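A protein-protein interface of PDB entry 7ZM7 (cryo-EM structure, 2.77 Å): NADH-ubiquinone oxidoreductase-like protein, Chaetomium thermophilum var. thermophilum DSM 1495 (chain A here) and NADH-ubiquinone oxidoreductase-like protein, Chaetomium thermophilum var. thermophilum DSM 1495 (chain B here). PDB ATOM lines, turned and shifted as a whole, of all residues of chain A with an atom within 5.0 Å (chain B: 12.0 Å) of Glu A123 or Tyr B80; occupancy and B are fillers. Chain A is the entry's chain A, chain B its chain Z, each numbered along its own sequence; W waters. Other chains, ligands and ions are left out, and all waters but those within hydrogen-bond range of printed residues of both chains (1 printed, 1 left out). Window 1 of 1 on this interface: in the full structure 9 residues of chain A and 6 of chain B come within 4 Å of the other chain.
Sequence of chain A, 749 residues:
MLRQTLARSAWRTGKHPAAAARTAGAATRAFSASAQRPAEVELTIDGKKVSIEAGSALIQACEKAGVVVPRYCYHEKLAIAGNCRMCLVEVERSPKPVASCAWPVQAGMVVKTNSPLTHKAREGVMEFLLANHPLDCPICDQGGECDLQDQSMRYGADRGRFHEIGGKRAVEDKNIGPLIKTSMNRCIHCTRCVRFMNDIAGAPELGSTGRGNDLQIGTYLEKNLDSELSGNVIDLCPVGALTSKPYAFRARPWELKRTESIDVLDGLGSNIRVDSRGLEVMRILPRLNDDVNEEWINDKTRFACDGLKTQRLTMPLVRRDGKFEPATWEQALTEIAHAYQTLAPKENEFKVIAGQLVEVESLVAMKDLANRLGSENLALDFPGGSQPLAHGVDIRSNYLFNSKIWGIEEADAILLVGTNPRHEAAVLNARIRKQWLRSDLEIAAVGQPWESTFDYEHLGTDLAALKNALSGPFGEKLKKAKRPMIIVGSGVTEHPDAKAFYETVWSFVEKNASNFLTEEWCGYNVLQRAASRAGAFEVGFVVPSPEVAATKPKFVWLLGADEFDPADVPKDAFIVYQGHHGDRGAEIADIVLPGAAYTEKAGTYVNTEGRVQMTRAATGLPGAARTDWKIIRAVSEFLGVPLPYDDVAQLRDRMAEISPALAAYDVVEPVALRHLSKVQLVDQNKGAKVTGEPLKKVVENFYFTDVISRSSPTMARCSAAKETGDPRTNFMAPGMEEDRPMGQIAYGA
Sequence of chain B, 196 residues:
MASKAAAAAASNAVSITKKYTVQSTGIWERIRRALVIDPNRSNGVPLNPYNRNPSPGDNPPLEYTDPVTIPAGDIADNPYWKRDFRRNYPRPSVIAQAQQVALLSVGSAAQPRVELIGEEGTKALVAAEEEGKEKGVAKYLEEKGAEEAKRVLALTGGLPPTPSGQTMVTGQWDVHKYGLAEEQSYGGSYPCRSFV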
ATOM      1  N   HIS A 119      -8.209  25.624  -6.934  1.00  0.00           N
ATOM      2  CA  HIS A 119      -6.921  25.787  -6.269  1.00  0.00           C
ATOM      3  C   HIS A 119      -7.082  25.931  -4.768  1.00  0.00           C
ATOM      4  O   HIS A 119      -6.403  25.245  -3.999  1.00  0.00           O
ATOM      5  CB  HIS A 119      -6.172  26.992  -6.819  1.00  0.00           C
ATOM      6  CG  HIS A 119      -5.566  26.771  -8.161  1.00  0.00           C
ATOM      7  ND1 HIS A 119      -5.235  27.809  -8.997  1.00  0.00           N
ATOM      8  CD2 HIS A 119      -5.234  25.638  -8.817  1.00  0.00           C
ATOM      9  CE1 HIS A 119      -4.718  27.325 -10.109  1.00  0.00           C
ATOM     10  NE2 HIS A 119      -4.713  26.009 -10.027  1.00  0.00           N
ATOM     11  N   LYS A 120      -7.970  26.815  -4.321  1.00  0.00           N
ATOM     12  CA  LYS A 120      -8.107  26.962  -2.880  1.00  0.00           C
ATOM     13  C   LYS A 120      -8.817  25.777  -2.258  1.00  0.00           C
ATOM     14  O   LYS A 120      -8.694  25.565  -1.054  1.00  0.00           O
ATOM     15  CB  LYS A 120      -8.841  28.240  -2.508  1.00  0.00           C
ATOM     16  CG  LYS A 120     -10.321  28.186  -2.612  1.00  0.00           C
ATOM     17  CD  LYS A 120     -10.907  29.526  -2.225  1.00  0.00           C
ATOM     18  CE  LYS A 120     -10.705  29.820  -0.749  1.00  0.00           C
ATOM     19  NZ  LYS A 120     -11.506  28.917   0.113  1.00  0.00           N
ATOM     20  N   ALA A 121      -9.573  25.012  -3.042  1.00  0.00           N
ATOM     21  CA  ALA A 121     -10.166  23.791  -2.525  1.00  0.00           C
ATOM     22  C   ALA A 121      -9.086  22.782  -2.169  1.00  0.00           C
ATOM     23  O   ALA A 121      -9.118  22.179  -1.095  1.00  0.00           O
ATOM     24  CB  ALA A 121     -11.147  23.214  -3.538  1.00  0.00           C
ATOM     25  N   ARG A 122      -8.096  22.624  -3.043  1.00  0.00           N
ATOM     26  CA  ARG A 122      -7.108  21.573  -2.859  1.00  0.00           C
ATOM     27  C   ARG A 122      -6.129  21.914  -1.751  1.00  0.00           C
ATOM     28  O   ARG A 122      -5.682  21.025  -1.021  1.00  0.00           O
ATOM     29  CB  ARG A 122      -6.375  21.312  -4.168  1.00  0.00           C
ATOM     30  CG  ARG A 122      -7.228  20.748  -5.242  1.00  0.00           C
ATOM     31  CD  ARG A 122      -6.555  20.881  -6.567  1.00  0.00           C
ATOM     32  NE  ARG A 122      -7.322  20.240  -7.615  1.00  0.00           N
ATOM     33  CZ  ARG A 122      -6.926  20.143  -8.871  1.00  0.00           C
ATOM     34  NH1 ARG A 122      -5.779  20.657  -9.243  1.00  0.00           N
ATOM     35  NH2 ARG A 122      -7.686  19.530  -9.758  1.00  0.00           N
ATOM     36  N   GLU A 123      -5.774  23.189  -1.613  1.00  0.00           N
ATOM     37  CA  GLU A 123      -4.907  23.602  -0.517  1.00  0.00           C
ATOM     38  C   GLU A 123      -5.602  23.447   0.823  1.00  0.00           C
ATOM     39  O   GLU A 123      -4.973  23.070   1.814  1.00  0.00           O
ATOM     40  CB  GLU A 123      -4.459  25.044  -0.717  1.00  0.00           C
ATOM     41  CG  GLU A 123      -3.614  25.260  -1.940  1.00  0.00           C
ATOM     42  CD  GLU A 123      -2.755  26.489  -1.851  1.00  0.00           C
ATOM     43  OE1 GLU A 123      -2.529  26.981  -0.731  1.00  0.00           O
ATOM     44  OE2 GLU A 123      -2.295  26.969  -2.901  1.00  0.00           O
ATOM     45  N   GLY A 124      -6.897  23.740   0.874  1.00  0.00           N
ATOM     46  CA  GLY A 124      -7.631  23.598   2.117  1.00  0.00           C
ATOM     47  C   GLY A 124      -7.746  22.161   2.574  1.00  0.00           C
ATOM     48  O   GLY A 124      -7.659  21.870   3.765  1.00  0.00           O
ATOM     49  N   VAL A 125      -7.949  21.241   1.637  1.00  0.00           N
ATOM     50  CA  VAL A 125      -7.988  19.832   1.990  1.00  0.00           C
ATOM     51  C   VAL A 125      -6.603  19.342   2.376  1.00  0.00           C
ATOM     52  O   VAL A 125      -6.442  18.590   3.341  1.00  0.00           O
ATOM     53  CB  VAL A 125      -8.597  19.018   0.838  1.00  0.00           C
ATOM     54  CG1 VAL A 125      -8.317  17.545   1.006  1.00  0.00           C
ATOM     55  CG2 VAL A 125     -10.075  19.254   0.792  1.00  0.00           C
ATOM     56  N   MET A 126      -5.579  19.761   1.638  1.00  0.00           N
ATOM     57  CA  MET A 126      -4.227  19.346   1.970  1.00  0.00           C
ATOM     58  C   MET A 126      -3.785  19.901   3.312  1.00  0.00           C
ATOM     59  O   MET A 126      -2.944  19.299   3.976  1.00  0.00           O
ATOM     60  CB  MET A 126      -3.256  19.771   0.876  1.00  0.00           C
ATOM     61  CG  MET A 126      -3.069  18.757  -0.235  1.00  0.00           C
ATOM     62  SD  MET A 126      -3.160  17.038   0.270  1.00  0.00           S
ATOM     63  CE  MET A 126      -1.645  16.892   1.188  1.00  0.00           C
ATOM     64  N   GLU A 127      -4.335  21.036   3.732  1.00  0.00           N
ATOM     65  CA  GLU A 127      -4.028  21.556   5.055  1.00  0.00           C
ATOM     66  C   GLU A 127      -4.717  20.745   6.144  1.00  0.00           C
ATOM     67  O   GLU A 127      -4.166  20.559   7.228  1.00  0.00           O
ATOM     68  CB  GLU A 127      -4.420  23.026   5.130  1.00  0.00           C
ATOM     69  CG  GLU A 127      -3.933  23.726   6.365  1.00  0.00           C
ATOM     70  CD  GLU A 127      -3.495  25.144   6.125  1.00  0.00           C
ATOM     71  OE1 GLU A 127      -4.170  25.855   5.360  1.00  0.00           O
ATOM     72  OE2 GLU A 127      -2.480  25.549   6.724  1.00  0.00           O
ATOM     73  N   TYR A 155      -0.212  20.127  -4.892  1.00  0.00           N
ATOM     74  CA  TYR A 155      -1.478  20.819  -4.733  1.00  0.00           C
ATOM     75  C   TYR A 155      -1.656  21.488  -3.385  1.00  0.00           C
ATOM     76  O   TYR A 155      -2.673  22.150  -3.179  1.00  0.00           O
ATOM     77  CB  TYR A 155      -2.641  19.852  -4.977  1.00  0.00           C
ATOM     78  CG  TYR A 155      -2.564  19.223  -6.327  1.00  0.00           C
ATOM     79  CD1 TYR A 155      -2.804  19.960  -7.465  1.00  0.00           C
ATOM     80  CD2 TYR A 155      -2.211  17.896  -6.469  1.00  0.00           C
ATOM     81  CE1 TYR A 155      -2.713  19.392  -8.695  1.00  0.00           C
ATOM     82  CE2 TYR A 155      -2.115  17.325  -7.688  1.00  0.00           C
ATOM     83  CZ  TYR A 155      -2.364  18.073  -8.800  1.00  0.00           C
ATOM     84  OH  TYR A 155      -2.266  17.483 -10.028  1.00  0.00           O
ATOM     85  N   GLY A 156      -0.702  21.360  -2.468  1.00  0.00           N
ATOM     86  CA  GLY A 156      -0.808  21.967  -1.164  1.00  0.00           C
ATOM     87  C   GLY A 156      -0.074  23.292  -1.072  1.00  0.00           C
ATOM     88  O   GLY A 156       0.431  23.833  -2.053  1.00  0.00           O
ATOM     89  N   ALA A 157      -0.029  23.821   0.139  1.00  0.00           N
ATOM     90  CA  ALA A 157       0.833  24.945   0.453  1.00  0.00           C
ATOM     91  C   ALA A 157       2.214  24.451   0.846  1.00  0.00           C
ATOM     92  O   ALA A 157       2.402  23.298   1.236  1.00  0.00           O
ATOM     93  CB  ALA A 157       0.257  25.782   1.582  1.00  0.00           C
ATOM     94  N   ASP A 158       3.191  25.346   0.727  1.00  0.00           N
ATOM     95  CA  ASP A 158       4.574  24.990   0.994  1.00  0.00           C
ATOM     96  C   ASP A 158       4.875  24.880   2.477  1.00  0.00           C
ATOM     97  O   ASP A 158       5.829  24.197   2.847  1.00  0.00           O
ATOM     98  CB  ASP A 158       5.518  25.999   0.340  1.00  0.00           C
ATOM     99  CG  ASP A 158       5.468  27.364   0.996  1.00  0.00           C
ATOM    100  OD1 ASP A 158       4.364  27.828   1.337  1.00  0.00           O
ATOM    101  OD2 ASP A 158       6.540  27.977   1.178  1.00  0.00           O
ATOM    102  N   THR B  69       8.901  37.367   5.597  1.00  0.00           N
ATOM    103  CA  THR B  69       8.286  38.556   5.030  1.00  0.00           C
ATOM    104  C   THR B  69       6.780  38.391   4.991  1.00  0.00           C
ATOM    105  O   THR B  69       6.271  37.314   4.683  1.00  0.00           O
ATOM    106  CB  THR B  69       8.804  38.854   3.626  1.00  0.00           C
ATOM    107  OG1 THR B  69       8.511  37.751   2.761  1.00  0.00           O
ATOM    108  CG2 THR B  69      10.281  39.119   3.646  1.00  0.00           C
ATOM    109  N   ILE B  70       6.077  39.485   5.255  1.00  0.00           N
ATOM    110  CA  ILE B  70       4.652  39.397   5.564  1.00  0.00           C
ATOM    111  C   ILE B  70       3.846  38.689   4.484  1.00  0.00           C
ATOM    112  O   ILE B  70       3.107  37.751   4.821  1.00  0.00           O
ATOM    113  CB  ILE B  70       4.097  40.795   5.888  1.00  0.00           C
ATOM    114  CG1 ILE B  70       4.702  41.267   7.203  1.00  0.00           C
ATOM    115  CG2 ILE B  70       2.588  40.775   5.909  1.00  0.00           C
ATOM    116  CD1 ILE B  70       4.445  40.307   8.326  1.00  0.00           C
ATOM    117  N   PRO B  71       3.932  39.054   3.201  1.00  0.00           N
ATOM    118  CA  PRO B  71       3.059  38.378   2.228  1.00  0.00           C
ATOM    119  C   PRO B  71       3.254  36.876   2.262  1.00  0.00           C
ATOM    120  O   PRO B  71       2.333  36.156   2.639  1.00  0.00           O
ATOM    121  CB  PRO B  71       3.486  38.974   0.880  1.00  0.00           C
ATOM    122  CG  PRO B  71       4.081  40.282   1.239  1.00  0.00           C
ATOM    123  CD  PRO B  71       4.756  40.095   2.568  1.00  0.00           C
ATOM    124  N   ALA B  72       4.469  36.409   1.960  1.00  0.00           N
ATOM    125  CA  ALA B  72       4.741  34.994   1.736  1.00  0.00           C
ATOM    126  C   ALA B  72       4.821  34.162   3.008  1.00  0.00           C
ATOM    127  O   ALA B  72       4.515  32.968   2.964  1.00  0.00           O
ATOM    128  CB  ALA B  72       6.041  34.832   0.958  1.00  0.00           C
ATOM    129  N   GLY B  73       5.217  34.750   4.129  1.00  0.00           N
ATOM    130  CA  GLY B  73       5.337  34.044   5.382  1.00  0.00           C
ATOM    131  C   GLY B  73       4.197  34.231   6.353  1.00  0.00           C
ATOM    132  O   GLY B  73       4.306  33.775   7.497  1.00  0.00           O
ATOM    133  N   ASP B  74       3.098  34.864   5.946  1.00  0.00           N
ATOM    134  CA  ASP B  74       2.027  35.103   6.896  1.00  0.00           C
ATOM    135  C   ASP B  74       1.175  33.863   7.096  1.00  0.00           C
ATOM    136  O   ASP B  74       1.230  32.907   6.330  1.00  0.00           O
ATOM    137  CB  ASP B  74       1.128  36.252   6.460  1.00  0.00           C
ATOM    138  CG  ASP B  74       0.403  36.899   7.637  1.00  0.00           C
ATOM    139  OD1 ASP B  74       0.921  36.820   8.770  1.00  0.00           O
ATOM    140  OD2 ASP B  74      -0.675  37.483   7.438  1.00  0.00           O
ATOM    141  N   ILE B  75       0.369  33.899   8.153  1.00  0.00           N
ATOM    142  CA  ILE B  75      -0.536  32.808   8.469  1.00  0.00           C
ATOM    143  C   ILE B  75      -1.947  33.032   7.952  1.00  0.00           C
ATOM    144  O   ILE B  75      -2.747  32.089   7.964  1.00  0.00           O
ATOM    145  CB  ILE B  75      -0.597  32.570   9.992  1.00  0.00           C
ATOM    146  CG1 ILE B  75      -1.263  33.756  10.681  1.00  0.00           C
ATOM    147  CG2 ILE B  75       0.780  32.353  10.551  1.00  0.00           C
ATOM    148  CD1 ILE B  75      -1.424  33.596  12.148  1.00  0.00           C
ATOM    149  N   ALA B  76      -2.286  34.234   7.498  1.00  0.00           N
ATOM    150  CA  ALA B  76      -3.699  34.526   7.348  1.00  0.00           C
ATOM    151  C   ALA B  76      -4.130  35.246   6.084  1.00  0.00           C
ATOM    152  O   ALA B  76      -5.334  35.449   5.932  1.00  0.00           O
ATOM    153  CB  ALA B  76      -4.186  35.340   8.546  1.00  0.00           C
ATOM    154  N   ASP B  77      -3.244  35.697   5.211  1.00  0.00           N
ATOM    155  CA  ASP B  77      -3.703  36.357   3.989  1.00  0.00           C
ATOM    156  C   ASP B  77      -2.805  36.018   2.807  1.00  0.00           C
ATOM    157  O   ASP B  77      -2.385  36.893   2.052  1.00  0.00           O
ATOM    158  CB  ASP B  77      -3.786  37.869   4.179  1.00  0.00           C
ATOM    159  CG  ASP B  77      -5.143  38.320   4.670  1.00  0.00           C
ATOM    160  OD1 ASP B  77      -6.152  37.719   4.253  1.00  0.00           O
ATOM    161  OD2 ASP B  77      -5.200  39.275   5.472  1.00  0.00           O
ATOM    162  N   ASN B  78      -2.474  34.752   2.639  1.00  0.00           N
ATOM    163  CA  ASN B  78      -1.647  34.335   1.511  1.00  0.00           C
ATOM    164  C   ASN B  78      -2.014  32.922   1.094  1.00  0.00           C
ATOM    165  O   ASN B  78      -1.585  31.934   1.705  1.00  0.00           O
ATOM    166  CB  ASN B  78      -0.156  34.493   1.810  1.00  0.00           C
ATOM    167  CG  ASN B  78       0.369  33.528   2.826  1.00  0.00           C
ATOM    168  OD1 ASN B  78       1.129  32.633   2.501  1.00  0.00           O
ATOM    169  ND2 ASN B  78      -0.127  33.631   4.040  1.00  0.00           N
ATOM    170  N   PRO B  79      -2.858  32.789   0.080  1.00  0.00           N
ATOM    171  CA  PRO B  79      -2.985  31.503  -0.603  1.00  0.00           C
ATOM    172  C   PRO B  79      -1.762  31.239  -1.464  1.00  0.00           C
ATOM    173  O   PRO B  79      -1.279  32.119  -2.172  1.00  0.00           O
ATOM    174  CB  PRO B  79      -4.243  31.681  -1.449  1.00  0.00           C
ATOM    175  CG  PRO B  79      -4.361  33.101  -1.623  1.00  0.00           C
ATOM    176  CD  PRO B  79      -3.833  33.767  -0.412  1.00  0.00           C
ATOM    177  N   TYR B  80      -1.261  30.014  -1.398  1.00  0.00           N
ATOM    178  CA  TYR B  80      -0.004  29.718  -2.065  1.00  0.00           C
ATOM    179  C   TYR B  80      -0.096  29.925  -3.570  1.00  0.00           C
ATOM    180  O   TYR B  80       0.902  30.270  -4.207  1.00  0.00           O
ATOM    181  CB  TYR B  80       0.437  28.289  -1.758  1.00  0.00           C
ATOM    182  CG  TYR B  80       1.668  27.895  -2.516  1.00  0.00           C
ATOM    183  CD1 TYR B  80       2.902  28.359  -2.130  1.00  0.00           C
ATOM    184  CD2 TYR B  80       1.591  27.113  -3.655  1.00  0.00           C
ATOM    185  CE1 TYR B  80       4.013  28.034  -2.824  1.00  0.00           C
ATOM    186  CE2 TYR B  80       2.717  26.783  -4.361  1.00  0.00           C
ATOM    187  CZ  TYR B  80       3.928  27.248  -3.931  1.00  0.00           C
ATOM    188  OH  TYR B  80       5.070  26.937  -4.607  1.00  0.00           O
ATOM    189  N   TRP B  81      -1.284  29.766  -4.152  1.00  0.00           N
ATOM    190  CA  TRP B  81      -1.380  29.720  -5.600  1.00  0.00           C
ATOM    191  C   TRP B  81      -1.295  31.094  -6.251  1.00  0.00           C
ATOM    192  O   TRP B  81      -1.128  31.156  -7.470  1.00  0.00           O
ATOM    193  CB  TRP B  81      -2.668  29.011  -6.026  1.00  0.00           C
ATOM    194  CG  TRP B  81      -3.941  29.744  -5.733  1.00  0.00           C
ATOM    195  CD1 TRP B  81      -4.779  29.547  -4.683  1.00  0.00           C
ATOM    196  CD2 TRP B  81      -4.556  30.731  -6.552  1.00  0.00           C
ATOM    197  NE1 TRP B  81      -5.855  30.381  -4.775  1.00  0.00           N
ATOM    198  CE2 TRP B  81      -5.738  31.122  -5.917  1.00  0.00           C
ATOM    199  CE3 TRP B  81      -4.207  31.343  -7.758  1.00  0.00           C
ATOM    200  CZ2 TRP B  81      -6.578  32.077  -6.451  1.00  0.00           C
ATOM    201  CZ3 TRP B  81      -5.039  32.294  -8.276  1.00  0.00           C
ATOM    202  CH2 TRP B  81      -6.203  32.657  -7.623  1.00  0.00           C
ATOM    203  N   LYS B  82      -1.397  32.193  -5.494  1.00  0.00           N
ATOM    204  CA  LYS B  82      -1.009  33.485  -6.056  1.00  0.00           C
ATOM    205  C   LYS B  82       0.495  33.633  -6.171  1.00  0.00           C
ATOM    206  O   LYS B  82       0.970  34.375  -7.032  1.00  0.00           O
ATOM    207  CB  LYS B  82      -1.500  34.671  -5.236  1.00  0.00           C
ATOM    208  CG  LYS B  82      -2.923  35.151  -5.377  1.00  0.00           C
ATOM    209  CD  LYS B  82      -3.957  34.294  -4.758  1.00  0.00           C
ATOM    210  CE  LYS B  82      -5.302  34.980  -4.899  1.00  0.00           C
ATOM    211  NZ  LYS B  82      -6.440  34.173  -4.406  1.00  0.00           N
ATOM    212  N   ARG B  83       1.260  32.991  -5.289  1.00  0.00           N
ATOM    213  CA  ARG B  83       2.702  33.165  -5.257  1.00  0.00           C
ATOM    214  C   ARG B  83       3.453  31.956  -5.813  1.00  0.00           C
ATOM    215  O   ARG B  83       4.621  31.747  -5.475  1.00  0.00           O
ATOM    216  CB  ARG B  83       3.159  33.485  -3.832  1.00  0.00           C
ATOM    217  CG  ARG B  83       2.974  32.389  -2.814  1.00  0.00           C
ATOM    218  CD  ARG B  83       3.438  32.800  -1.457  1.00  0.00           C
ATOM    219  NE  ARG B  83       3.106  31.810  -0.446  1.00  0.00           N
ATOM    220  CZ  ARG B  83       3.974  30.948   0.066  1.00  0.00           C
ATOM    221  NH1 ARG B  83       3.579  30.079   0.983  1.00  0.00           N
ATOM    222  NH2 ARG B  83       5.241  30.954  -0.332  1.00  0.00           N
ATOM    223  N   ASP B  84       2.810  31.156  -6.659  1.00  0.00           N
ATOM    224  CA  ASP B  84       3.452  29.999  -7.289  1.00  0.00           C
ATOM    225  C   ASP B  84       3.894  30.356  -8.702  1.00  0.00           C
ATOM    226  O   ASP B  84       3.315  29.944  -9.693  1.00  0.00           O
ATOM    227  CB  ASP B  84       2.508  28.806  -7.294  1.00  0.00           C
ATOM    228  CG  ASP B  84       3.183  27.521  -7.741  1.00  0.00           C
ATOM    229  OD1 ASP B  84       4.425  27.433  -7.697  1.00  0.00           O
ATOM    230  OD2 ASP B  84       2.454  26.571  -8.101  1.00  0.00           O
ATOM    231  N   PHE B  85       4.963  31.127  -8.776  1.00  0.00           N
ATOM    232  CA  PHE B  85       5.427  31.599 -10.065  1.00  0.00           C
ATOM    233  C   PHE B  85       6.205  30.545 -10.825  1.00  0.00           C
ATOM    234  O   PHE B  85       6.433  30.705 -12.024  1.00  0.00           O
ATOM    235  CB  PHE B  85       6.275  32.843  -9.872  1.00  0.00           C
ATOM    236  CG  PHE B  85       5.565  33.942  -9.172  1.00  0.00           C
ATOM    237  CD1 PHE B  85       4.546  34.617  -9.786  1.00  0.00           C
ATOM    238  CD2 PHE B  85       5.898  34.284  -7.887  1.00  0.00           C
ATOM    239  CE1 PHE B  85       3.899  35.617  -9.143  1.00  0.00           C
ATOM    240  CE2 PHE B  85       5.235  35.290  -7.244  1.00  0.00           C
ATOM    241  CZ  PHE B  85       4.250  35.958  -7.877  1.00  0.00           C
ATOM    242  N   ARG B  86       6.620  29.478 -10.157  1.00  0.00           N
ATOM    243  CA  ARG B  86       7.262  28.385 -10.862  1.00  0.00           C
ATOM    244  C   ARG B  86       6.275  27.655 -11.751  1.00  0.00           C
ATOM    245  O   ARG B  86       6.641  27.165 -12.819  1.00  0.00           O
ATOM    246  CB  ARG B  86       7.903  27.420  -9.876  1.00  0.00           C
ATOM    247  CG  ARG B  86       8.654  26.318 -10.566  1.00  0.00           C
ATOM    248  CD  ARG B  86       9.244  25.390  -9.609  1.00  0.00           C
ATOM    249  NE  ARG B  86       8.270  24.841  -8.682  1.00  0.00           N
ATOM    250  CZ  ARG B  86       8.334  23.608  -8.210  1.00  0.00           C
ATOM    251  NH1 ARG B  86       7.431  23.176  -7.359  1.00  0.00           N
ATOM    252  NH2 ARG B  86       9.315  22.819  -8.595  1.00  0.00           N
ATOM    253  N   ARG B  87       5.026  27.565 -11.332  1.00  0.00           N
ATOM    254  CA  ARG B  87       4.028  26.897 -12.138  1.00  0.00           C
ATOM    255  C   ARG B  87       3.271  27.854 -13.035  1.00  0.00           C
ATOM    256  O   ARG B  87       2.413  27.415 -13.801  1.00  0.00           O
ATOM    257  CB  ARG B  87       3.081  26.112 -11.245  1.00  0.00           C
ATOM    258  CG  ARG B  87       3.761  24.896 -10.702  1.00  0.00           C
ATOM    259  CD  ARG B  87       2.807  23.918 -10.134  1.00  0.00           C
ATOM    260  NE  ARG B  87       3.491  22.963  -9.278  1.00  0.00           N
ATOM    261  CZ  ARG B  87       3.412  22.971  -7.960  1.00  0.00           C
ATOM    262  NH1 ARG B  87       2.694  23.893  -7.353  1.00  0.00           N
ATOM    263  NH2 ARG B  87       4.059  22.063  -7.255  1.00  0.00           N
ATOM    264  N   ASN B  88       3.577  29.145 -12.971  1.00  0.00           N
ATOM    265  CA  ASN B  88       3.151  30.100 -13.980  1.00  0.00           C
ATOM    266  C   ASN B  88       4.301  30.497 -14.881  1.00  0.00           C
ATOM    267  O   ASN B  88       4.489  31.676 -15.174  1.00  0.00           O
ATOM    268  CB  ASN B  88       2.511  31.326 -13.335  1.00  0.00           C
ATOM    269  CG  ASN B  88       1.142  31.037 -12.795  1.00  0.00           C
ATOM    270  OD1 ASN B  88       0.953  30.125 -12.004  1.00  0.00           O
ATOM    271  ND2 ASN B  88       0.174  31.814 -13.225  1.00  0.00           N
ATOM    272  N   TYR B  89       5.082  29.529 -15.297  1.00  0.00           N
ATOM    273  CA  TYR B  89       6.249  29.786 -16.114  1.00  0.00           C
ATOM    274  C   TYR B  89       5.838  30.055 -17.553  1.00  0.00           C
ATOM    275  O   TYR B  89       4.824  29.518 -18.011  1.00  0.00           O
ATOM    276  CB  TYR B  89       7.210  28.604 -16.028  1.00  0.00           C
ATOM    277  CG  TYR B  89       6.769  27.309 -16.676  1.00  0.00           C
ATOM    278  CD1 TYR B  89       6.100  26.332 -15.950  1.00  0.00           C
ATOM    279  CD2 TYR B  89       7.078  27.035 -17.996  1.00  0.00           C
ATOM    280  CE1 TYR B  89       5.736  25.143 -16.534  1.00  0.00           C
ATOM    281  CE2 TYR B  89       6.709  25.866 -18.584  1.00  0.00           C
ATOM    282  CZ  TYR B  89       6.048  24.919 -17.855  1.00  0.00           C
ATOM    283  OH  TYR B  89       5.685  23.747 -18.463  1.00  0.00           O
HETATM  284  O   HOH W   1       0.434  24.158  -4.991  1.00  0.00           O
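The side-chain carboxylate of Glu A123 lies within hydrogen-bond range of the backbone NH of Tyr B80 (3.4 Å).
N of Trp B81 lies within hydrogen-bond range of OE2 of Glu A123 (3.2 Å).
NH1 of Arg B83 lies within salt-bridge range of OD1 of Asp A158, at 2.4 Å.
The side-chain hydroxyl (OH) of Tyr B80 lies within hydrogen-bond range of the side-chain carboxylate (OD1) of Asp B84 (3.2 Å).
Among the printed residues, pairs that only touch across the chains: His A119 with Trp B81 (3.6 Å), Asp A158 with Tyr B80 (3.8 Å) and Gly A156 with Tyr B80 (3.8 Å).
His A119 touches just one residue of chain B: Trp B81.
No residue of chain B comes within 4 Å of Ala A121.
No residue of chain B comes within 4 Å of Gly A124.
No residue of chain B comes within 4 Å of Met A126.
No residue of chain B comes within 4 Å of Glu A127.
Of chain B, only Tyr B80 comes within 4 Å of Gly A156.
No residue of chain B comes within 4 Å of Ala A157.
Printed residues of chain A within 4 Å of Trp B81: His A119 and Glu A123.
Of the printed residues of chain A, Arg B83 touches Asp A158.
Printed residues of chain A that touch a printed residue of chain B: His A119, Glu A123, Gly A156 and Asp A158.
Hydrophobic or aromatic side chains of chain A within 4 Å of the printed part of chain B: His A119.
Hydrophobic or aromatic side chains of chain B within 4 Å of the printed part of chain A: Tyr B80 and Trp B81.
Among the printed residues, Asp or Glu carboxylates within 4 Å of a Lys or Arg side-chain nitrogen of the other chain: Asp A158 with Arg B83 (2.4 Å).
Water W1 lies within hydrogen-bond range of O of Gly A156 and NH1 of Arg B87.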
